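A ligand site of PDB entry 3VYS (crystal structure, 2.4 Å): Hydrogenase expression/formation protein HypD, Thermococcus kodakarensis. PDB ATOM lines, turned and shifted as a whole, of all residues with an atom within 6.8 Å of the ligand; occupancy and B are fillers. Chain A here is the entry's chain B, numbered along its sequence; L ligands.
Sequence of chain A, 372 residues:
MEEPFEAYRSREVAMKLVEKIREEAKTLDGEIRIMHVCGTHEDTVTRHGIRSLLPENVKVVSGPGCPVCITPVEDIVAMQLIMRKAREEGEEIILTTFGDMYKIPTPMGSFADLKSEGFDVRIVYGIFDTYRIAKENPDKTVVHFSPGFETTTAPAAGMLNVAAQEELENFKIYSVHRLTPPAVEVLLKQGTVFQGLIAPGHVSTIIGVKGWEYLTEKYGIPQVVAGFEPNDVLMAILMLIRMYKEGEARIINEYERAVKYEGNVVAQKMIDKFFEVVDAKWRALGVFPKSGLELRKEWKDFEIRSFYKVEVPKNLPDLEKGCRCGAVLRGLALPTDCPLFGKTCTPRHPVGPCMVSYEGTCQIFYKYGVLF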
ATOM      1  N   LEU A 319     -21.040  -8.096   3.269  1.00  0.00           N
ATOM      2  CA  LEU A 319     -20.204  -8.825   2.321  1.00  0.00           C
ATOM      3  C   LEU A 319     -18.950  -8.073   1.920  1.00  0.00           C
ATOM      4  O   LEU A 319     -18.887  -6.854   2.031  1.00  0.00           O
ATOM      5  CB  LEU A 319     -21.003  -9.113   1.039  1.00  0.00           C
ATOM      6  CG  LEU A 319     -22.312  -9.894   1.079  1.00  0.00           C
ATOM      7  CD1 LEU A 319     -22.983  -9.853  -0.289  1.00  0.00           C
ATOM      8  CD2 LEU A 319     -22.054 -11.328   1.490  1.00  0.00           C
ATOM      9  N   GLU A 320     -17.945  -8.816   1.442  1.00  0.00           N
ATOM     10  CA  GLU A 320     -16.708  -8.201   0.986  1.00  0.00           C
ATOM     11  C   GLU A 320     -17.022  -7.480  -0.328  1.00  0.00           C
ATOM     12  O   GLU A 320     -17.946  -7.857  -1.032  1.00  0.00           O
ATOM     13  CB  GLU A 320     -15.639  -9.278   0.740  1.00  0.00           C
ATOM     14  CG  GLU A 320     -15.019  -9.853   2.010  1.00  0.00           C
ATOM     15  CD  GLU A 320     -14.128  -8.848   2.726  1.00  0.00           C
ATOM     16  OE1 GLU A 320     -13.607  -9.182   3.823  1.00  0.00           O
ATOM     17  OE2 GLU A 320     -13.941  -7.734   2.205  1.00  0.00           O
ATOM     18  N   LYS A 321     -16.255  -6.450  -0.638  1.00  0.00           N
ATOM     19  CA  LYS A 321     -16.479  -5.706  -1.865  1.00  0.00           C
ATOM     20  C   LYS A 321     -16.362  -6.648  -3.057  1.00  0.00           C
ATOM     21  O   LYS A 321     -15.435  -7.453  -3.135  1.00  0.00           O
ATOM     22  CB  LYS A 321     -15.462  -4.583  -1.985  1.00  0.00           C
ATOM     23  N   GLY A 322     -17.311  -6.568  -3.982  1.00  0.00           N
ATOM     24  CA  GLY A 322     -17.272  -7.412  -5.151  1.00  0.00           C
ATOM     25  C   GLY A 322     -18.135  -8.650  -5.048  1.00  0.00           C
ATOM     26  O   GLY A 322     -18.467  -9.264  -6.063  1.00  0.00           O
ATOM     27  N   CYS A 323     -18.500  -9.032  -3.833  1.00  0.00           N
ATOM     28  CA  CYS A 323     -19.330 -10.204  -3.606  1.00  0.00           C
ATOM     29  C   CYS A 323     -20.774  -9.925  -4.002  1.00  0.00           C
ATOM     30  O   CYS A 323     -21.340  -8.908  -3.604  1.00  0.00           O
ATOM     31  CB  CYS A 323     -19.242 -10.626  -2.150  1.00  0.00           C
ATOM     32  SG  CYS A 323     -20.242 -12.081  -1.722  1.00  0.00           S
ATOM     33  N   ARG A 324     -21.359 -10.833  -4.772  1.00  0.00           N
ATOM     34  CA  ARG A 324     -22.737 -10.680  -5.229  1.00  0.00           C
ATOM     35  C   ARG A 324     -23.637 -11.794  -4.699  1.00  0.00           C
ATOM     36  O   ARG A 324     -24.606 -12.188  -5.342  1.00  0.00           O
ATOM     37  CB  ARG A 324     -22.746 -10.618  -6.749  1.00  0.00           C
ATOM     38  CG  ARG A 324     -22.048  -9.342  -7.235  1.00  0.00           C
ATOM     39  CD  ARG A 324     -21.409  -9.409  -8.600  1.00  0.00           C
ATOM     40  NE  ARG A 324     -22.374  -9.544  -9.684  1.00  0.00           N
ATOM     41  CZ  ARG A 324     -22.151  -9.128 -10.930  1.00  0.00           C
ATOM     42  NH1 ARG A 324     -21.004  -8.552 -11.246  1.00  0.00           N
ATOM     43  NH2 ARG A 324     -23.084  -9.306 -11.856  1.00  0.00           N
ATOM     44  N   CYS A 325     -23.311 -12.286  -3.504  1.00  0.00           N
ATOM     45  CA  CYS A 325     -24.053 -13.355  -2.845  1.00  0.00           C
ATOM     46  C   CYS A 325     -25.480 -12.922  -2.491  1.00  0.00           C
ATOM     47  O   CYS A 325     -26.391 -13.746  -2.401  1.00  0.00           O
ATOM     48  CB  CYS A 325     -23.255 -13.802  -1.604  1.00  0.00           C
ATOM     49  SG  CYS A 325     -23.993 -15.045  -0.486  1.00  0.00           S
ATOM     50  N   GLY A 326     -25.658 -11.622  -2.284  1.00  0.00           N
ATOM     51  CA  GLY A 326     -26.985 -11.106  -1.980  1.00  0.00           C
ATOM     52  C   GLY A 326     -27.913 -11.340  -3.164  1.00  0.00           C
ATOM     53  O   GLY A 326     -29.049 -11.800  -2.992  1.00  0.00           O
ATOM     54  N   VAL A 328     -27.356 -13.503  -5.597  1.00  0.00           N
ATOM     55  CA  VAL A 328     -27.387 -14.942  -5.830  1.00  0.00           C
ATOM     56  C   VAL A 328     -28.499 -15.544  -4.976  1.00  0.00           C
ATOM     57  O   VAL A 328     -29.255 -16.425  -5.421  1.00  0.00           O
ATOM     58  CB  VAL A 328     -26.043 -15.592  -5.436  1.00  0.00           C
ATOM     59  CG1 VAL A 328     -26.235 -17.088  -5.172  1.00  0.00           C
ATOM     60  CG2 VAL A 328     -25.000 -15.369  -6.541  1.00  0.00           C
ATOM     61  N   LEU A 334     -26.432 -15.382 -10.917  1.00  0.00           N
ATOM     62  CA  LEU A 334     -25.791 -16.690 -10.957  1.00  0.00           C
ATOM     63  C   LEU A 334     -24.370 -16.500 -10.423  1.00  0.00           C
ATOM     64  O   LEU A 334     -23.798 -15.435 -10.581  1.00  0.00           O
ATOM     65  CB  LEU A 334     -25.732 -17.212 -12.399  1.00  0.00           C
ATOM     66  CG  LEU A 334     -27.051 -17.501 -13.114  1.00  0.00           C
ATOM     67  CD1 LEU A 334     -26.786 -17.720 -14.584  1.00  0.00           C
ATOM     68  CD2 LEU A 334     -27.708 -18.728 -12.505  1.00  0.00           C
ATOM     69  N   PRO A 335     -23.795 -17.535  -9.787  1.00  0.00           N
ATOM     70  CA  PRO A 335     -22.436 -17.460  -9.242  1.00  0.00           C
ATOM     71  C   PRO A 335     -21.433 -16.986 -10.293  1.00  0.00           C
ATOM     72  O   PRO A 335     -20.552 -16.169 -10.027  1.00  0.00           O
ATOM     73  CB  PRO A 335     -22.164 -18.889  -8.791  1.00  0.00           C
ATOM     74  CG  PRO A 335     -23.500 -19.392  -8.426  1.00  0.00           C
ATOM     75  CD  PRO A 335     -24.391 -18.865  -9.532  1.00  0.00           C
ATOM     76  N   ASP A 337     -21.841 -15.000 -12.634  1.00  0.00           N
ATOM     77  CA  ASP A 337     -21.951 -13.576 -12.952  1.00  0.00           C
ATOM     78  C   ASP A 337     -20.943 -12.828 -12.083  1.00  0.00           C
ATOM     79  O   ASP A 337     -20.546 -11.707 -12.383  1.00  0.00           O
ATOM     80  CB  ASP A 337     -23.344 -13.012 -12.653  1.00  0.00           C
ATOM     81  CG  ASP A 337     -24.428 -13.590 -13.537  1.00  0.00           C
ATOM     82  OD1 ASP A 337     -24.109 -14.147 -14.606  1.00  0.00           O
ATOM     83  OD2 ASP A 337     -25.618 -13.471 -13.154  1.00  0.00           O
ATOM     84  N   CYS A 338     -20.565 -13.450 -10.989  1.00  0.00           N
ATOM     85  CA  CYS A 338     -19.635 -12.821 -10.066  1.00  0.00           C
ATOM     86  C   CYS A 338     -18.187 -12.862 -10.575  1.00  0.00           C
ATOM     87  O   CYS A 338     -17.706 -13.895 -11.025  1.00  0.00           O
ATOM     88  CB  CYS A 338     -19.719 -13.508  -8.711  1.00  0.00           C
ATOM     89  SG  CYS A 338     -18.534 -12.835  -7.518  1.00  0.00           S
ATOM     90  N   PRO A 339     -17.473 -11.732 -10.488  1.00  0.00           N
ATOM     91  CA  PRO A 339     -16.090 -11.677 -10.955  1.00  0.00           C
ATOM     92  C   PRO A 339     -15.105 -12.487 -10.106  1.00  0.00           C
ATOM     93  O   PRO A 339     -14.070 -12.958 -10.609  1.00  0.00           O
ATOM     94  CB  PRO A 339     -15.776 -10.177 -10.937  1.00  0.00           C
ATOM     95  CG  PRO A 339     -16.615  -9.691  -9.774  1.00  0.00           C
ATOM     96  CD  PRO A 339     -17.926 -10.418  -9.995  1.00  0.00           C
ATOM     97  N   LEU A 340     -15.410 -12.656  -8.822  1.00  0.00           N
ATOM     98  CA  LEU A 340     -14.528 -13.381  -7.917  1.00  0.00           C
ATOM     99  C   LEU A 340     -14.721 -14.889  -8.013  1.00  0.00           C
ATOM    100  O   LEU A 340     -13.795 -15.658  -7.734  1.00  0.00           O
ATOM    101  CB  LEU A 340     -14.793 -12.922  -6.481  1.00  0.00           C
ATOM    102  CG  LEU A 340     -14.906 -11.402  -6.365  1.00  0.00           C
ATOM    103  CD1 LEU A 340     -14.982 -10.982  -4.899  1.00  0.00           C
ATOM    104  CD2 LEU A 340     -13.700 -10.761  -7.030  1.00  0.00           C
ATOM    105  N   PHE A 341     -15.896 -15.304  -8.441  1.00  0.00           N
ATOM    106  CA  PHE A 341     -16.213 -16.719  -8.579  1.00  0.00           C
ATOM    107  C   PHE A 341     -15.138 -17.536  -9.291  1.00  0.00           C
ATOM    108  O   PHE A 341     -14.820 -17.290 -10.454  1.00  0.00           O
ATOM    109  CB  PHE A 341     -17.521 -16.863  -9.343  1.00  0.00           C
ATOM    110  CG  PHE A 341     -17.928 -18.288  -9.601  1.00  0.00           C
ATOM    111  CD1 PHE A 341     -18.615 -19.018  -8.652  1.00  0.00           C
ATOM    112  CD2 PHE A 341     -17.640 -18.883 -10.820  1.00  0.00           C
ATOM    113  CE1 PHE A 341     -19.015 -20.313  -8.902  1.00  0.00           C
ATOM    114  CE2 PHE A 341     -18.042 -20.192 -11.076  1.00  0.00           C
ATOM    115  CZ  PHE A 341     -18.739 -20.901 -10.119  1.00  0.00           C
ATOM    116  N   GLY A 342     -14.554 -18.494  -8.583  1.00  0.00           N
ATOM    117  CA  GLY A 342     -13.553 -19.361  -9.167  1.00  0.00           C
ATOM    118  C   GLY A 342     -12.210 -18.686  -9.342  1.00  0.00           C
ATOM    119  O   GLY A 342     -11.296 -19.256  -9.929  1.00  0.00           O
ATOM    120  N   THR A 344     -10.663 -15.427  -6.899  1.00  0.00           N
ATOM    121  CA  THR A 344     -10.228 -15.192  -5.526  1.00  0.00           C
ATOM    122  C   THR A 344     -11.193 -15.872  -4.578  1.00  0.00           C
ATOM    123  O   THR A 344     -10.918 -15.995  -3.397  1.00  0.00           O
ATOM    124  CB  THR A 344     -10.149 -13.699  -5.180  1.00  0.00           C
ATOM    125  OG1 THR A 344     -11.434 -13.096  -5.342  1.00  0.00           O
ATOM    126  CG2 THR A 344      -9.161 -12.997  -6.093  1.00  0.00           C
ATOM    127  N   CYS A 345     -12.321 -16.332  -5.107  1.00  0.00           N
ATOM    128  CA  CYS A 345     -13.315 -16.983  -4.272  1.00  0.00           C
ATOM    129  C   CYS A 345     -13.559 -18.432  -4.665  1.00  0.00           C
ATOM    130  O   CYS A 345     -14.083 -18.729  -5.738  1.00  0.00           O
ATOM    131  CB  CYS A 345     -14.624 -16.198  -4.348  1.00  0.00           C
ATOM    132  SG  CYS A 345     -15.880 -16.744  -3.136  1.00  0.00           S
ATOM    133  N   THR A 346     -13.163 -19.327  -3.780  1.00  0.00           N
ATOM    134  CA  THR A 346     -13.348 -20.758  -3.999  1.00  0.00           C
ATOM    135  C   THR A 346     -13.728 -21.352  -2.651  1.00  0.00           C
ATOM    136  O   THR A 346     -13.628 -20.676  -1.624  1.00  0.00           O
ATOM    137  CB  THR A 346     -12.062 -21.460  -4.525  1.00  0.00           C
ATOM    138  OG1 THR A 346     -11.006 -21.286  -3.580  1.00  0.00           O
ATOM    139  CG2 THR A 346     -11.642 -20.866  -5.879  1.00  0.00           C
ATOM    140  N   PRO A 350     -12.754 -18.986   0.368  1.00  0.00           N
ATOM    141  CA  PRO A 350     -13.967 -18.221   0.089  1.00  0.00           C
ATOM    142  C   PRO A 350     -13.939 -16.758   0.478  1.00  0.00           C
ATOM    143  O   PRO A 350     -13.360 -16.378   1.494  1.00  0.00           O
ATOM    144  CB  PRO A 350     -15.043 -18.992   0.844  1.00  0.00           C
ATOM    145  CG  PRO A 350     -14.301 -19.474   2.055  1.00  0.00           C
ATOM    146  CD  PRO A 350     -12.976 -19.930   1.475  1.00  0.00           C
ATOM    147  N   VAL A 351     -14.583 -15.946  -0.359  1.00  0.00           N
ATOM    148  CA  VAL A 351     -14.684 -14.521  -0.102  1.00  0.00           C
ATOM    149  C   VAL A 351     -16.038 -14.217   0.512  1.00  0.00           C
ATOM    150  O   VAL A 351     -16.151 -13.415   1.440  1.00  0.00           O
ATOM    151  CB  VAL A 351     -14.541 -13.722  -1.407  1.00  0.00           C
ATOM    152  CG1 VAL A 351     -14.677 -12.232  -1.116  1.00  0.00           C
ATOM    153  CG2 VAL A 351     -13.184 -14.037  -2.051  1.00  0.00           C
ATOM    154  N   GLY A 352     -17.076 -14.878  -0.004  1.00  0.00           N
ATOM    155  CA  GLY A 352     -18.428 -14.669   0.492  1.00  0.00           C
ATOM    156  C   GLY A 352     -19.036 -15.901   1.138  1.00  0.00           C
ATOM    157  O   GLY A 352     -18.473 -16.989   1.056  1.00  0.00           O
ATOM    158  N   PRO A 353     -20.189 -15.745   1.797  1.00  0.00           N
ATOM    159  CA  PRO A 353     -20.850 -16.881   2.466  1.00  0.00           C
ATOM    160  C   PRO A 353     -21.476 -17.901   1.519  1.00  0.00           C
ATOM    161  O   PRO A 353     -21.542 -19.081   1.848  1.00  0.00           O
ATOM    162  CB  PRO A 353     -21.875 -16.201   3.371  1.00  0.00           C
ATOM    163  CG  PRO A 353     -22.200 -14.934   2.632  1.00  0.00           C
ATOM    164  CD  PRO A 353     -20.855 -14.478   2.127  1.00  0.00           C
ATOM    165  N   CYS A 354     -21.909 -17.463   0.343  1.00  0.00           N
ATOM    166  CA  CYS A 354     -22.511 -18.383  -0.622  1.00  0.00           C
ATOM    167  C   CYS A 354     -21.557 -19.495  -1.082  1.00  0.00           C
ATOM    168  O   CYS A 354     -21.999 -20.557  -1.501  1.00  0.00           O
ATOM    169  CB  CYS A 354     -23.012 -17.614  -1.848  1.00  0.00           C
ATOM    170  SG  CYS A 354     -24.519 -16.617  -1.662  1.00  0.00           S
ATOM    171  N   MET A 355     -20.251 -19.243  -0.996  1.00  0.00           N
ATOM    172  CA  MET A 355     -19.260 -20.221  -1.414  1.00  0.00           C
ATOM    173  C   MET A 355     -18.821 -21.115  -0.244  1.00  0.00           C
ATOM    174  O   MET A 355     -18.407 -22.250  -0.450  1.00  0.00           O
ATOM    175  CB  MET A 355     -18.030 -19.510  -1.998  1.00  0.00           C
ATOM    176  CG  MET A 355     -16.965 -20.430  -2.598  1.00  0.00           C
ATOM    177  SD  MET A 355     -17.477 -21.252  -4.137  1.00  0.00           S
ATOM    178  CE  MET A 355     -17.042 -20.029  -5.339  1.00  0.00           C
ATOM    179  N   VAL A 356     -18.918 -20.594   0.964  1.00  0.00           N
ATOM    180  CA  VAL A 356     -18.519 -21.343   2.147  1.00  0.00           C
ATOM    181  C   VAL A 356     -19.497 -22.452   2.507  1.00  0.00           C
ATOM    182  O   VAL A 356     -19.098 -23.593   2.772  1.00  0.00           O
ATOM    183  CB  VAL A 356     -18.424 -20.432   3.398  1.00  0.00           C
ATOM    184  CG1 VAL A 356     -18.055 -21.251   4.606  1.00  0.00           C
ATOM    185  CG2 VAL A 356     -17.418 -19.359   3.167  1.00  0.00           C
ATOM    186  N   THR A 361     -25.205 -21.612  -2.980  1.00  0.00           N
ATOM    187  CA  THR A 361     -25.342 -21.785  -4.416  1.00  0.00           C
ATOM    188  C   THR A 361     -23.987 -21.664  -5.113  1.00  0.00           C
ATOM    189  O   THR A 361     -23.721 -22.386  -6.079  1.00  0.00           O
ATOM    190  CB  THR A 361     -26.334 -20.751  -4.964  1.00  0.00           C
ATOM    191  OG1 THR A 361     -27.596 -20.932  -4.291  1.00  0.00           O
ATOM    192  CG2 THR A 361     -26.535 -20.943  -6.466  1.00  0.00           C
ATOM    193  N   CYS A 362     -23.136 -20.775  -4.619  1.00  0.00           N
ATOM    194  CA  CYS A 362     -21.807 -20.593  -5.202  1.00  0.00           C
ATOM    195  C   CYS A 362     -20.951 -21.836  -5.014  1.00  0.00           C
ATOM    196  O   CYS A 362     -20.249 -22.258  -5.942  1.00  0.00           O
ATOM    197  CB  CYS A 362     -21.134 -19.377  -4.585  1.00  0.00           C
ATOM    198  SG  CYS A 362     -21.921 -17.816  -5.086  1.00  0.00           S
ATOM    199  N   GLN A 363     -20.981 -22.424  -3.822  1.00  0.00           N
ATOM    200  CA  GLN A 363     -20.186 -23.619  -3.588  1.00  0.00           C
ATOM    201  C   GLN A 363     -20.676 -24.739  -4.495  1.00  0.00           C
ATOM    202  O   GLN A 363     -19.884 -25.442  -5.123  1.00  0.00           O
ATOM    203  CB  GLN A 363     -20.255 -24.058  -2.129  1.00  0.00           C
ATOM    204  CG  GLN A 363     -19.515 -25.372  -1.879  1.00  0.00           C
ATOM    205  CD  GLN A 363     -19.336 -25.698  -0.411  1.00  0.00           C
ATOM    206  OE1 GLN A 363     -19.862 -26.688   0.091  1.00  0.00           O
ATOM    207  NE2 GLN A 363     -18.586 -24.848   0.279  1.00  0.00           N
HETATM  208 FE1  LIG L   1     -20.473 -16.217  -4.705  1.00  0.00          FE
HETATM  209 FE2  LIG L   1     -18.994 -14.203  -5.775  1.00  0.00          FE
HETATM  210 FE3  LIG L   1     -19.806 -13.918  -3.046  1.00  0.00          FE
HETATM  211 FE4  LIG L   1     -17.845 -15.690  -3.664  1.00  0.00          FE
HETATM  212  S1  LIG L   1     -17.639 -13.764  -3.812  1.00  0.00           S
HETATM  213  S2  LIG L   1     -19.380 -16.140  -2.502  1.00  0.00           S
HETATM  214  S3  LIG L   1     -18.432 -16.401  -5.489  1.00  0.00           S
HETATM  215  S4  LIG L   1     -21.033 -13.994  -4.663  1.00  0.00           S
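Residues that only touch the ligand: Phe 341 (3.8 Å), Val 351 (3.9 Å), Cys 354 (3.97 Å) and Leu 340 (3.99 Å).
Hydrophobic or aromatic side chains that line the ligand: Leu 340, Phe 341, Val 351 and Met 355.
Of the 30 residues printed, 12 come within 4 Å of the ligand.
The nearest printed residue that does not touch the ligand is Pro 353 (4.4 Å).
SG of Cys 362 is bound to FE1 of the ligand, 2.2 Å away.
SG of Cys 338 binds FE2 of the ligand.
FE4 of the ligand is bound by SG of Cys 345 (2.3 Å).
SG of Cys 323 binds FE3 of the ligand, at 2.3 Å.
A sulfur (S4) of the ligand sits close to the backbone NH (N) of Cys 325, at 3.1 Å.
A sulfur (S4) of the ligand lies close to the backbone NH (N) of Arg 324 (3.2 Å).
The backbone NH (N) of Gly 352 sits close to a sulfur (S2) of the ligand (3.6 Å).
The backbone NH (N) of Met 355 sits close to a sulfur (S2) of the ligand (3.6 Å).
The backbone NH (N) of Cys 362 sits at hydrogen-bond distance from the backbone carbonyl oxygen (O) of Cys 354, at 3.3 Å.
The side-chain sulfur (SG) of Cys 338 sits close to the backbone NH (N) of Phe 341 (3.7 Å).
The backbone NH (N) of Leu 340 lies close to the side-chain sulfur (SG) of Cys 338 (3.4 Å).
The backbone NH (N) of Val 351 sits close to the side-chain sulfur (SG) of Cys 345, 3.2 Å away.
The backbone NH (N) of Cys 345 sits at hydrogen-bond distance from the backbone carbonyl oxygen (O) of Leu 340 (3.1 Å).
The side-chain sulfur of Cys 323 sits close to the backbone NH of Cys 325, at 3.6 Å.
SG of Cys 354 is disulfide-bonded to SG of Cys 325 (2.0 Å).
The guanidinium group (NH1) of Arg 324 lies close to the backbone carbonyl oxygen (O) of Asp 337 (3.4 Å).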
